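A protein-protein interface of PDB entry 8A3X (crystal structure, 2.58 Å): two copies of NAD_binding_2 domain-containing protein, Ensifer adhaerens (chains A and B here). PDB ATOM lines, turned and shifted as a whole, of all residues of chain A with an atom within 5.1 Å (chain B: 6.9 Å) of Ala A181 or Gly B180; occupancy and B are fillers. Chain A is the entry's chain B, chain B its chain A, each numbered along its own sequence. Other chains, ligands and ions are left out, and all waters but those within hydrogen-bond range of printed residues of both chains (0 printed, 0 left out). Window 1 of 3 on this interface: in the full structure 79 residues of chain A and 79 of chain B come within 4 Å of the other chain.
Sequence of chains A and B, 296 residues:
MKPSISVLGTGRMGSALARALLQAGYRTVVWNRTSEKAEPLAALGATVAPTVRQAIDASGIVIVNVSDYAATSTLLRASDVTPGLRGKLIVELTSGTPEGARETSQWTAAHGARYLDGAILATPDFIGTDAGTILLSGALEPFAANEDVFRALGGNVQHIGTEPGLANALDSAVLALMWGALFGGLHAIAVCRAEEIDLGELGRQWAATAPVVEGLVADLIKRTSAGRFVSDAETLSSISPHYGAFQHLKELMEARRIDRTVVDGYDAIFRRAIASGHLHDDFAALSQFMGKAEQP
The backbone carbonyl oxygen (O) of Gly B180 sits close to the backbone carbonyl oxygen (O) of Gly A180 (3.2 Å).
The backbone carbonyl oxygen of Phe B183 sits close to a ring nitrogen (ND1) of His B187, at 3.4 Å.
O of Ala B181 touches CD2 of Leu A177 (3.5 Å).
Leu A177 touches Gly B185.
Gly A180 touches Gly B184.
Gly B180 touches Ala A181 (C to N, 3.6 Å).
N of Ala A181 touches N of Ala B181 (3.7 Å).
Leu A182 touches Leu B220.
Phe A183 touches Tyr B266.
Gly A184 touches Leu B177 (O to N, 3.6 Å).
CD2 of Leu B177 touches N of Gly A185 (3.5 Å).
OH of Tyr A266 touches CA of Gly B180, at 3.5 Å.
Of the printed residues of chain B, Leu A177 touches Ala B181 (3.5 Å), Gly B184 (3.5 Å) and Gly B185 (3.2 Å).
Ala A181 touches just these residues of chain B: Leu B177, Gly B180, Ala B181 and Val B213.
Printed residues of chain B within 4 Å of Phe A183: Tyr B266 (3.4 Å).
Printed residues of chain A within 4 Å of Ala B176: Gly A184.
Of the printed residues of chain A, Gly B184 touches Leu A177 and Gly A180.
Printed residues of chain A within 4 Å of Gly B185: Leu A177 (3.2 Å).
The nearest residue of chain A that does not touch Gly B180 is Leu A177 (5.0 Å).
Of the 10 printed residues of chain A, 8 touch a printed residue of chain B.
Printed residues of chain A that touch a printed residue of chain B: Leu A177, Gly A180, Ala A181, Leu A182, Phe A183, Gly A184, Gly A185 and Tyr A266.
Hydrophobic or aromatic side chains of chain A within 4 Å of the printed part of chain B: Leu A177, Ala A181, Phe A183 and Tyr A266.
Along chain A the printed residues that touch a printed residue of chain B span positions 177 to 266.
Among the printed residues, 19 pairs touch across the chains.
Among the printed residues, no Asp or Glu carboxylate lies within 4 Å of a Lys or Arg side-chain nitrogen of the other chain.
Gly A180 touches its own counterpart, Gly B180.
Gly A180 touches Ala B181, and with the chains exchanged Ala A181 touches Gly B180.
Gly A180 touches Tyr B266, and with the chains exchanged Tyr A266 touches Gly B180.
Phe A183 touches Tyr B266, and with the chains exchanged Tyr A266 touches Phe B183.
10 positions are printed for both chains.
Of the 19 pairs that touch across the chains among the printed residues, 16 have their exchanged pair printed and touching as well.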
ATOM      1  N   LEU A 177     -25.597  28.772   3.704  1.00  0.00           N
ATOM      2  CA  LEU A 177     -24.976  27.929   4.759  1.00  0.00           C
ATOM      3  C   LEU A 177     -25.968  26.844   5.179  1.00  0.00           C
ATOM      4  O   LEU A 177     -25.605  25.659   5.151  1.00  0.00           O
ATOM      5  CB  LEU A 177     -24.586  28.794   5.956  1.00  0.00           C
ATOM      6  CG  LEU A 177     -23.138  29.264   5.943  1.00  0.00           C
ATOM      7  CD1 LEU A 177     -22.920  30.448   6.869  1.00  0.00           C
ATOM      8  CD2 LEU A 177     -22.213  28.130   6.332  1.00  0.00           C
ATOM      9  N   MET A 178     -27.184  27.243   5.528  1.00  0.00           N
ATOM     10  CA  MET A 178     -28.220  26.308   6.005  1.00  0.00           C
ATOM     11  C   MET A 178     -28.404  25.176   4.978  1.00  0.00           C
ATOM     12  O   MET A 178     -28.414  23.999   5.385  1.00  0.00           O
ATOM     13  CB  MET A 178     -29.547  27.031   6.233  1.00  0.00           C
ATOM     14  CG  MET A 178     -30.595  26.115   6.830  1.00  0.00           C
ATOM     15  SD  MET A 178     -32.292  26.635   6.555  1.00  0.00           S
ATOM     16  CE  MET A 178     -32.371  26.742   4.767  1.00  0.00           C
ATOM     17  N   TRP A 179     -28.542  25.508   3.696  1.00  0.00           N
ATOM     18  CA  TRP A 179     -28.788  24.507   2.613  1.00  0.00           C
ATOM     19  C   TRP A 179     -27.541  23.640   2.376  1.00  0.00           C
ATOM     20  O   TRP A 179     -27.707  22.423   2.168  1.00  0.00           O
ATOM     21  CB  TRP A 179     -29.279  25.170   1.311  1.00  0.00           C
ATOM     22  CG  TRP A 179     -30.716  25.603   1.336  1.00  0.00           C
ATOM     23  CD1 TRP A 179     -31.802  24.854   1.690  1.00  0.00           C
ATOM     24  CD2 TRP A 179     -31.225  26.890   0.962  1.00  0.00           C
ATOM     25  NE1 TRP A 179     -32.943  25.598   1.601  1.00  0.00           N
ATOM     26  CE2 TRP A 179     -32.621  26.850   1.157  1.00  0.00           C
ATOM     27  CE3 TRP A 179     -30.633  28.070   0.509  1.00  0.00           C
ATOM     28  CZ2 TRP A 179     -33.438  27.955   0.930  1.00  0.00           C
ATOM     29  CZ3 TRP A 179     -31.440  29.158   0.262  1.00  0.00           C
ATOM     30  CH2 TRP A 179     -32.822  29.098   0.476  1.00  0.00           C
ATOM     31  N   GLY A 180     -26.345  24.235   2.423  1.00  0.00           N
ATOM     32  CA  GLY A 180     -25.063  23.500   2.378  1.00  0.00           C
ATOM     33  C   GLY A 180     -25.073  22.341   3.367  1.00  0.00           C
ATOM     34  O   GLY A 180     -24.894  21.174   2.949  1.00  0.00           O
ATOM     35  N   ALA A 181     -25.303  22.657   4.633  1.00  0.00           N
ATOM     36  CA  ALA A 181     -25.378  21.690   5.748  1.00  0.00           C
ATOM     37  C   ALA A 181     -26.456  20.647   5.452  1.00  0.00           C
ATOM     38  O   ALA A 181     -26.179  19.473   5.606  1.00  0.00           O
ATOM     39  CB  ALA A 181     -25.660  22.420   7.035  1.00  0.00           C
ATOM     40  N   LEU A 182     -27.646  21.063   5.039  1.00  0.00           N
ATOM     41  CA  LEU A 182     -28.815  20.152   4.909  1.00  0.00           C
ATOM     42  C   LEU A 182     -28.601  19.181   3.742  1.00  0.00           C
ATOM     43  O   LEU A 182     -28.951  17.964   3.861  1.00  0.00           O
ATOM     44  CB  LEU A 182     -30.080  20.989   4.720  1.00  0.00           C
ATOM     45  CG  LEU A 182     -30.761  21.409   6.022  1.00  0.00           C
ATOM     46  CD1 LEU A 182     -31.692  22.594   5.796  1.00  0.00           C
ATOM     47  CD2 LEU A 182     -31.512  20.234   6.631  1.00  0.00           C
ATOM     48  N   PHE A 183     -28.055  19.689   2.637  1.00  0.00           N
ATOM     49  CA  PHE A 183     -27.786  18.864   1.434  1.00  0.00           C
ATOM     50  C   PHE A 183     -26.563  17.996   1.747  1.00  0.00           C
ATOM     51  O   PHE A 183     -26.486  16.870   1.222  1.00  0.00           O
ATOM     52  CB  PHE A 183     -27.700  19.746   0.184  1.00  0.00           C
ATOM     53  CG  PHE A 183     -29.057  20.019  -0.408  1.00  0.00           C
ATOM     54  CD1 PHE A 183     -29.669  19.079  -1.216  1.00  0.00           C
ATOM     55  CD2 PHE A 183     -29.754  21.173  -0.100  1.00  0.00           C
ATOM     56  CE1 PHE A 183     -30.931  19.308  -1.740  1.00  0.00           C
ATOM     57  CE2 PHE A 183     -31.020  21.390  -0.614  1.00  0.00           C
ATOM     58  CZ  PHE A 183     -31.602  20.462  -1.442  1.00  0.00           C
ATOM     59  N   GLY A 184     -25.675  18.495   2.615  1.00  0.00           N
ATOM     60  CA  GLY A 184     -24.604  17.715   3.266  1.00  0.00           C
ATOM     61  C   GLY A 184     -25.155  16.508   3.997  1.00  0.00           C
ATOM     62  O   GLY A 184     -24.597  15.418   3.809  1.00  0.00           O
ATOM     63  N   GLY A 185     -26.211  16.693   4.790  1.00  0.00           N
ATOM     64  CA  GLY A 185     -26.909  15.608   5.494  1.00  0.00           C
ATOM     65  C   GLY A 185     -27.516  14.629   4.511  1.00  0.00           C
ATOM     66  O   GLY A 185     -27.338  13.411   4.700  1.00  0.00           O
ATOM     67  N   TYR A 266     -18.452  21.016  -6.242  1.00  0.00           N
ATOM     68  CA  TYR A 266     -17.337  21.170  -5.271  1.00  0.00           C
ATOM     69  C   TYR A 266     -16.022  20.966  -6.033  1.00  0.00           C
ATOM     70  O   TYR A 266     -15.135  21.850  -6.003  1.00  0.00           O
ATOM     71  CB  TYR A 266     -17.371  20.165  -4.112  1.00  0.00           C
ATOM     72  CG  TYR A 266     -18.595  20.087  -3.229  1.00  0.00           C
ATOM     73  CD1 TYR A 266     -19.481  21.136  -3.053  1.00  0.00           C
ATOM     74  CD2 TYR A 266     -18.824  18.940  -2.492  1.00  0.00           C
ATOM     75  CE1 TYR A 266     -20.578  21.024  -2.205  1.00  0.00           C
ATOM     76  CE2 TYR A 266     -19.917  18.801  -1.656  1.00  0.00           C
ATOM     77  CZ  TYR A 266     -20.805  19.847  -1.505  1.00  0.00           C
ATOM     78  OH  TYR A 266     -21.872  19.671  -0.667  1.00  0.00           O
ATOM     79  N   LEU B 175     -17.933  13.336   6.666  1.00  0.00           N
ATOM     80  CA  LEU B 175     -17.206  14.329   5.834  1.00  0.00           C
ATOM     81  C   LEU B 175     -18.157  14.917   4.784  1.00  0.00           C
ATOM     82  O   LEU B 175     -17.924  16.070   4.376  1.00  0.00           O
ATOM     83  CB  LEU B 175     -15.979  13.669   5.187  1.00  0.00           C
ATOM     84  CG  LEU B 175     -14.619  13.998   5.813  1.00  0.00           C
ATOM     85  CD1 LEU B 175     -14.713  14.259   7.312  1.00  0.00           C
ATOM     86  CD2 LEU B 175     -13.618  12.891   5.527  1.00  0.00           C
ATOM     87  N   ALA B 176     -19.197  14.177   4.385  1.00  0.00           N
ATOM     88  CA  ALA B 176     -20.226  14.645   3.426  1.00  0.00           C
ATOM     89  C   ALA B 176     -20.954  15.861   4.021  1.00  0.00           C
ATOM     90  O   ALA B 176     -21.133  16.882   3.291  1.00  0.00           O
ATOM     91  CB  ALA B 176     -21.197  13.538   3.096  1.00  0.00           C
ATOM     92  N   LEU B 177     -21.355  15.735   5.293  1.00  0.00           N
ATOM     93  CA  LEU B 177     -21.960  16.817   6.108  1.00  0.00           C
ATOM     94  C   LEU B 177     -20.977  17.978   6.189  1.00  0.00           C
ATOM     95  O   LEU B 177     -21.370  19.104   5.874  1.00  0.00           O
ATOM     96  CB  LEU B 177     -22.294  16.280   7.503  1.00  0.00           C
ATOM     97  CG  LEU B 177     -23.754  15.858   7.667  1.00  0.00           C
ATOM     98  CD1 LEU B 177     -23.943  14.847   8.785  1.00  0.00           C
ATOM     99  CD2 LEU B 177     -24.620  17.077   7.903  1.00  0.00           C
ATOM    100  N   MET B 178     -19.747  17.697   6.593  1.00  0.00           N
ATOM    101  CA  MET B 178     -18.717  18.737   6.803  1.00  0.00           C
ATOM    102  C   MET B 178     -18.578  19.571   5.531  1.00  0.00           C
ATOM    103  O   MET B 178     -18.580  20.811   5.650  1.00  0.00           O
ATOM    104  CB  MET B 178     -17.369  18.111   7.156  1.00  0.00           C
ATOM    105  CG  MET B 178     -16.300  19.121   7.462  1.00  0.00           C
ATOM    106  SD  MET B 178     -14.659  18.374   7.319  1.00  0.00           S
ATOM    107  CE  MET B 178     -14.587  18.033   5.561  1.00  0.00           C
ATOM    108  N   TRP B 179     -18.471  18.934   4.360  1.00  0.00           N
ATOM    109  CA  TRP B 179     -18.256  19.646   3.066  1.00  0.00           C
ATOM    110  C   TRP B 179     -19.524  20.426   2.668  1.00  0.00           C
ATOM    111  O   TRP B 179     -19.379  21.567   2.175  1.00  0.00           O
ATOM    112  CB  TRP B 179     -17.799  18.686   1.959  1.00  0.00           C
ATOM    113  CG  TRP B 179     -16.364  18.267   2.038  1.00  0.00           C
ATOM    114  CD1 TRP B 179     -15.263  19.067   2.174  1.00  0.00           C
ATOM    115  CD2 TRP B 179     -15.867  16.922   1.951  1.00  0.00           C
ATOM    116  NE1 TRP B 179     -14.121  18.309   2.204  1.00  0.00           N
ATOM    117  CE2 TRP B 179     -14.460  16.991   2.066  1.00  0.00           C
ATOM    118  CE3 TRP B 179     -16.480  15.671   1.803  1.00  0.00           C
ATOM    119  CZ2 TRP B 179     -13.657  15.856   2.019  1.00  0.00           C
ATOM    120  CZ3 TRP B 179     -15.688  14.547   1.766  1.00  0.00           C
ATOM    121  CH2 TRP B 179     -14.298  14.643   1.886  1.00  0.00           C
ATOM    122  N   GLY B 180     -20.710  19.842   2.875  1.00  0.00           N
ATOM    123  CA  GLY B 180     -21.991  20.545   2.677  1.00  0.00           C
ATOM    124  C   GLY B 180     -21.988  21.909   3.365  1.00  0.00           C
ATOM    125  O   GLY B 180     -22.204  22.956   2.693  1.00  0.00           O
ATOM    126  N   ALA B 181     -21.725  21.897   4.670  1.00  0.00           N
ATOM    127  CA  ALA B 181     -21.653  23.096   5.527  1.00  0.00           C
ATOM    128  C   ALA B 181     -20.608  24.059   4.967  1.00  0.00           C
ATOM    129  O   ALA B 181     -20.916  25.246   4.849  1.00  0.00           O
ATOM    130  CB  ALA B 181     -21.323  22.689   6.935  1.00  0.00           C
ATOM    131  N   LEU B 182     -19.414  23.562   4.648  1.00  0.00           N
ATOM    132  CA  LEU B 182     -18.253  24.417   4.275  1.00  0.00           C
ATOM    133  C   LEU B 182     -18.513  25.079   2.922  1.00  0.00           C
ATOM    134  O   LEU B 182     -18.162  26.262   2.759  1.00  0.00           O
ATOM    135  CB  LEU B 182     -16.974  23.574   4.238  1.00  0.00           C
ATOM    136  CG  LEU B 182     -16.247  23.474   5.574  1.00  0.00           C
ATOM    137  CD1 LEU B 182     -15.290  22.302   5.581  1.00  0.00           C
ATOM    138  CD2 LEU B 182     -15.511  24.763   5.909  1.00  0.00           C
ATOM    139  N   PHE B 183     -19.083  24.341   1.975  1.00  0.00           N
ATOM    140  CA  PHE B 183     -19.387  24.868   0.627  1.00  0.00           C
ATOM    141  C   PHE B 183     -20.593  25.800   0.759  1.00  0.00           C
ATOM    142  O   PHE B 183     -20.666  26.777  -0.013  1.00  0.00           O
ATOM    143  CB  PHE B 183     -19.488  23.729  -0.393  1.00  0.00           C
ATOM    144  CG  PHE B 183     -18.136  23.339  -0.942  1.00  0.00           C
ATOM    145  CD1 PHE B 183     -17.536  24.093  -1.946  1.00  0.00           C
ATOM    146  CD2 PHE B 183     -17.436  22.266  -0.414  1.00  0.00           C
ATOM    147  CE1 PHE B 183     -16.287  23.755  -2.443  1.00  0.00           C
ATOM    148  CE2 PHE B 183     -16.182  21.942  -0.905  1.00  0.00           C
ATOM    149  CZ  PHE B 183     -15.603  22.691  -1.908  1.00  0.00           C
ATOM    150  N   GLY B 184     -21.459  25.530   1.742  1.00  0.00           N
ATOM    151  CA  GLY B 184     -22.501  26.467   2.212  1.00  0.00           C
ATOM    152  C   GLY B 184     -21.909  27.816   2.622  1.00  0.00           C
ATOM    153  O   GLY B 184     -22.435  28.881   2.194  1.00  0.00           O
ATOM    154  N   GLY B 185     -20.841  27.783   3.422  1.00  0.00           N
ATOM    155  CA  GLY B 185     -20.110  28.991   3.849  1.00  0.00           C
ATOM    156  C   GLY B 185     -19.486  29.697   2.659  1.00  0.00           C
ATOM    157  O   GLY B 185     -19.611  30.936   2.555  1.00  0.00           O
ATOM    158  N   HIS B 187     -20.402  29.712  -0.437  1.00  0.00           N
ATOM    159  CA  HIS B 187     -21.557  30.391  -1.085  1.00  0.00           C
ATOM    160  C   HIS B 187     -21.919  31.659  -0.303  1.00  0.00           C
ATOM    161  O   HIS B 187     -21.956  32.758  -0.924  1.00  0.00           O
ATOM    162  CB  HIS B 187     -22.766  29.460  -1.176  1.00  0.00           C
ATOM    163  CG  HIS B 187     -22.637  28.398  -2.214  1.00  0.00           C
ATOM    164  ND1 HIS B 187     -23.335  27.203  -2.133  1.00  0.00           N
ATOM    165  CD2 HIS B 187     -21.904  28.341  -3.349  1.00  0.00           C
ATOM    166  CE1 HIS B 187     -23.034  26.456  -3.180  1.00  0.00           C
ATOM    167  NE2 HIS B 187     -22.154  27.132  -3.936  1.00  0.00           N
ATOM    168  N   VAL B 213     -29.602  25.477  12.418  1.00  0.00           N
ATOM    169  CA  VAL B 213     -29.072  24.551  11.372  1.00  0.00           C
ATOM    170  C   VAL B 213     -28.836  23.175  12.012  1.00  0.00           C
ATOM    171  O   VAL B 213     -29.248  22.164  11.405  1.00  0.00           O
ATOM    172  CB  VAL B 213     -27.783  25.108  10.735  1.00  0.00           C
ATOM    173  CG1 VAL B 213     -27.261  24.171   9.663  1.00  0.00           C
ATOM    174  CG2 VAL B 213     -27.971  26.514  10.175  1.00  0.00           C
ATOM    175  N   GLU B 214     -28.224  23.141  13.202  1.00  0.00           N
ATOM    176  CA  GLU B 214     -27.985  21.890  13.971  1.00  0.00           C
ATOM    177  C   GLU B 214     -29.312  21.175  14.222  1.00  0.00           C
ATOM    178  O   GLU B 214     -29.389  19.969  13.947  1.00  0.00           O
ATOM    179  CB  GLU B 214     -27.255  22.149  15.286  1.00  0.00           C
ATOM    180  CG  GLU B 214     -25.810  22.604  15.091  1.00  0.00           C
ATOM    181  CD  GLU B 214     -24.901  22.424  16.295  1.00  0.00           C
ATOM    182  OE1 GLU B 214     -25.414  22.484  17.437  1.00  0.00           O
ATOM    183  OE2 GLU B 214     -23.692  22.219  16.078  1.00  0.00           O
ATOM    184  N   VAL B 217     -30.558  19.782  10.769  1.00  0.00           N
ATOM    185  CA  VAL B 217     -29.778  18.583  10.348  1.00  0.00           C
ATOM    186  C   VAL B 217     -30.208  17.374  11.198  1.00  0.00           C
ATOM    187  O   VAL B 217     -30.576  16.338  10.600  1.00  0.00           O
ATOM    188  CB  VAL B 217     -28.267  18.849  10.443  1.00  0.00           C
ATOM    189  CG1 VAL B 217     -27.469  17.566  10.245  1.00  0.00           C
ATOM    190  CG2 VAL B 217     -27.814  19.923   9.466  1.00  0.00           C
ATOM    191  N   LEU B 220     -33.663  16.232  10.095  1.00  0.00           N
ATOM    192  CA  LEU B 220     -33.476  15.506   8.809  1.00  0.00           C
ATOM    193  C   LEU B 220     -33.204  14.026   9.100  1.00  0.00           C
ATOM    194  O   LEU B 220     -33.971  13.159   8.615  1.00  0.00           O
ATOM    195  CB  LEU B 220     -32.290  16.118   8.055  1.00  0.00           C
ATOM    196  CG  LEU B 220     -32.349  16.082   6.529  1.00  0.00           C
ATOM    197  CD1 LEU B 220     -30.939  16.135   5.955  1.00  0.00           C
ATOM    198  CD2 LEU B 220     -33.106  14.870   5.991  1.00  0.00           C
ATOM    199  N   TYR B 266     -28.775  21.213  -6.101  1.00  0.00           N
ATOM    200  CA  TYR B 266     -29.871  21.281  -5.092  1.00  0.00           C
ATOM    201  C   TYR B 266     -31.205  21.352  -5.850  1.00  0.00           C
ATOM    202  O   TYR B 266     -32.096  20.519  -5.603  1.00  0.00           O
ATOM    203  CB  TYR B 266     -29.785  22.498  -4.158  1.00  0.00           C
ATOM    204  CG  TYR B 266     -28.518  22.736  -3.360  1.00  0.00           C
ATOM    205  CD1 TYR B 266     -27.633  21.731  -3.011  1.00  0.00           C
ATOM    206  CD2 TYR B 266     -28.241  24.010  -2.897  1.00  0.00           C
ATOM    207  CE1 TYR B 266     -26.492  21.995  -2.264  1.00  0.00           C
ATOM    208  CE2 TYR B 266     -27.104  24.293  -2.162  1.00  0.00           C
ATOM    209  CZ  TYR B 266     -26.229  23.280  -1.823  1.00  0.00           C
ATOM    210  OH  TYR B 266     -25.124  23.604  -1.080  1.00  0.00           O
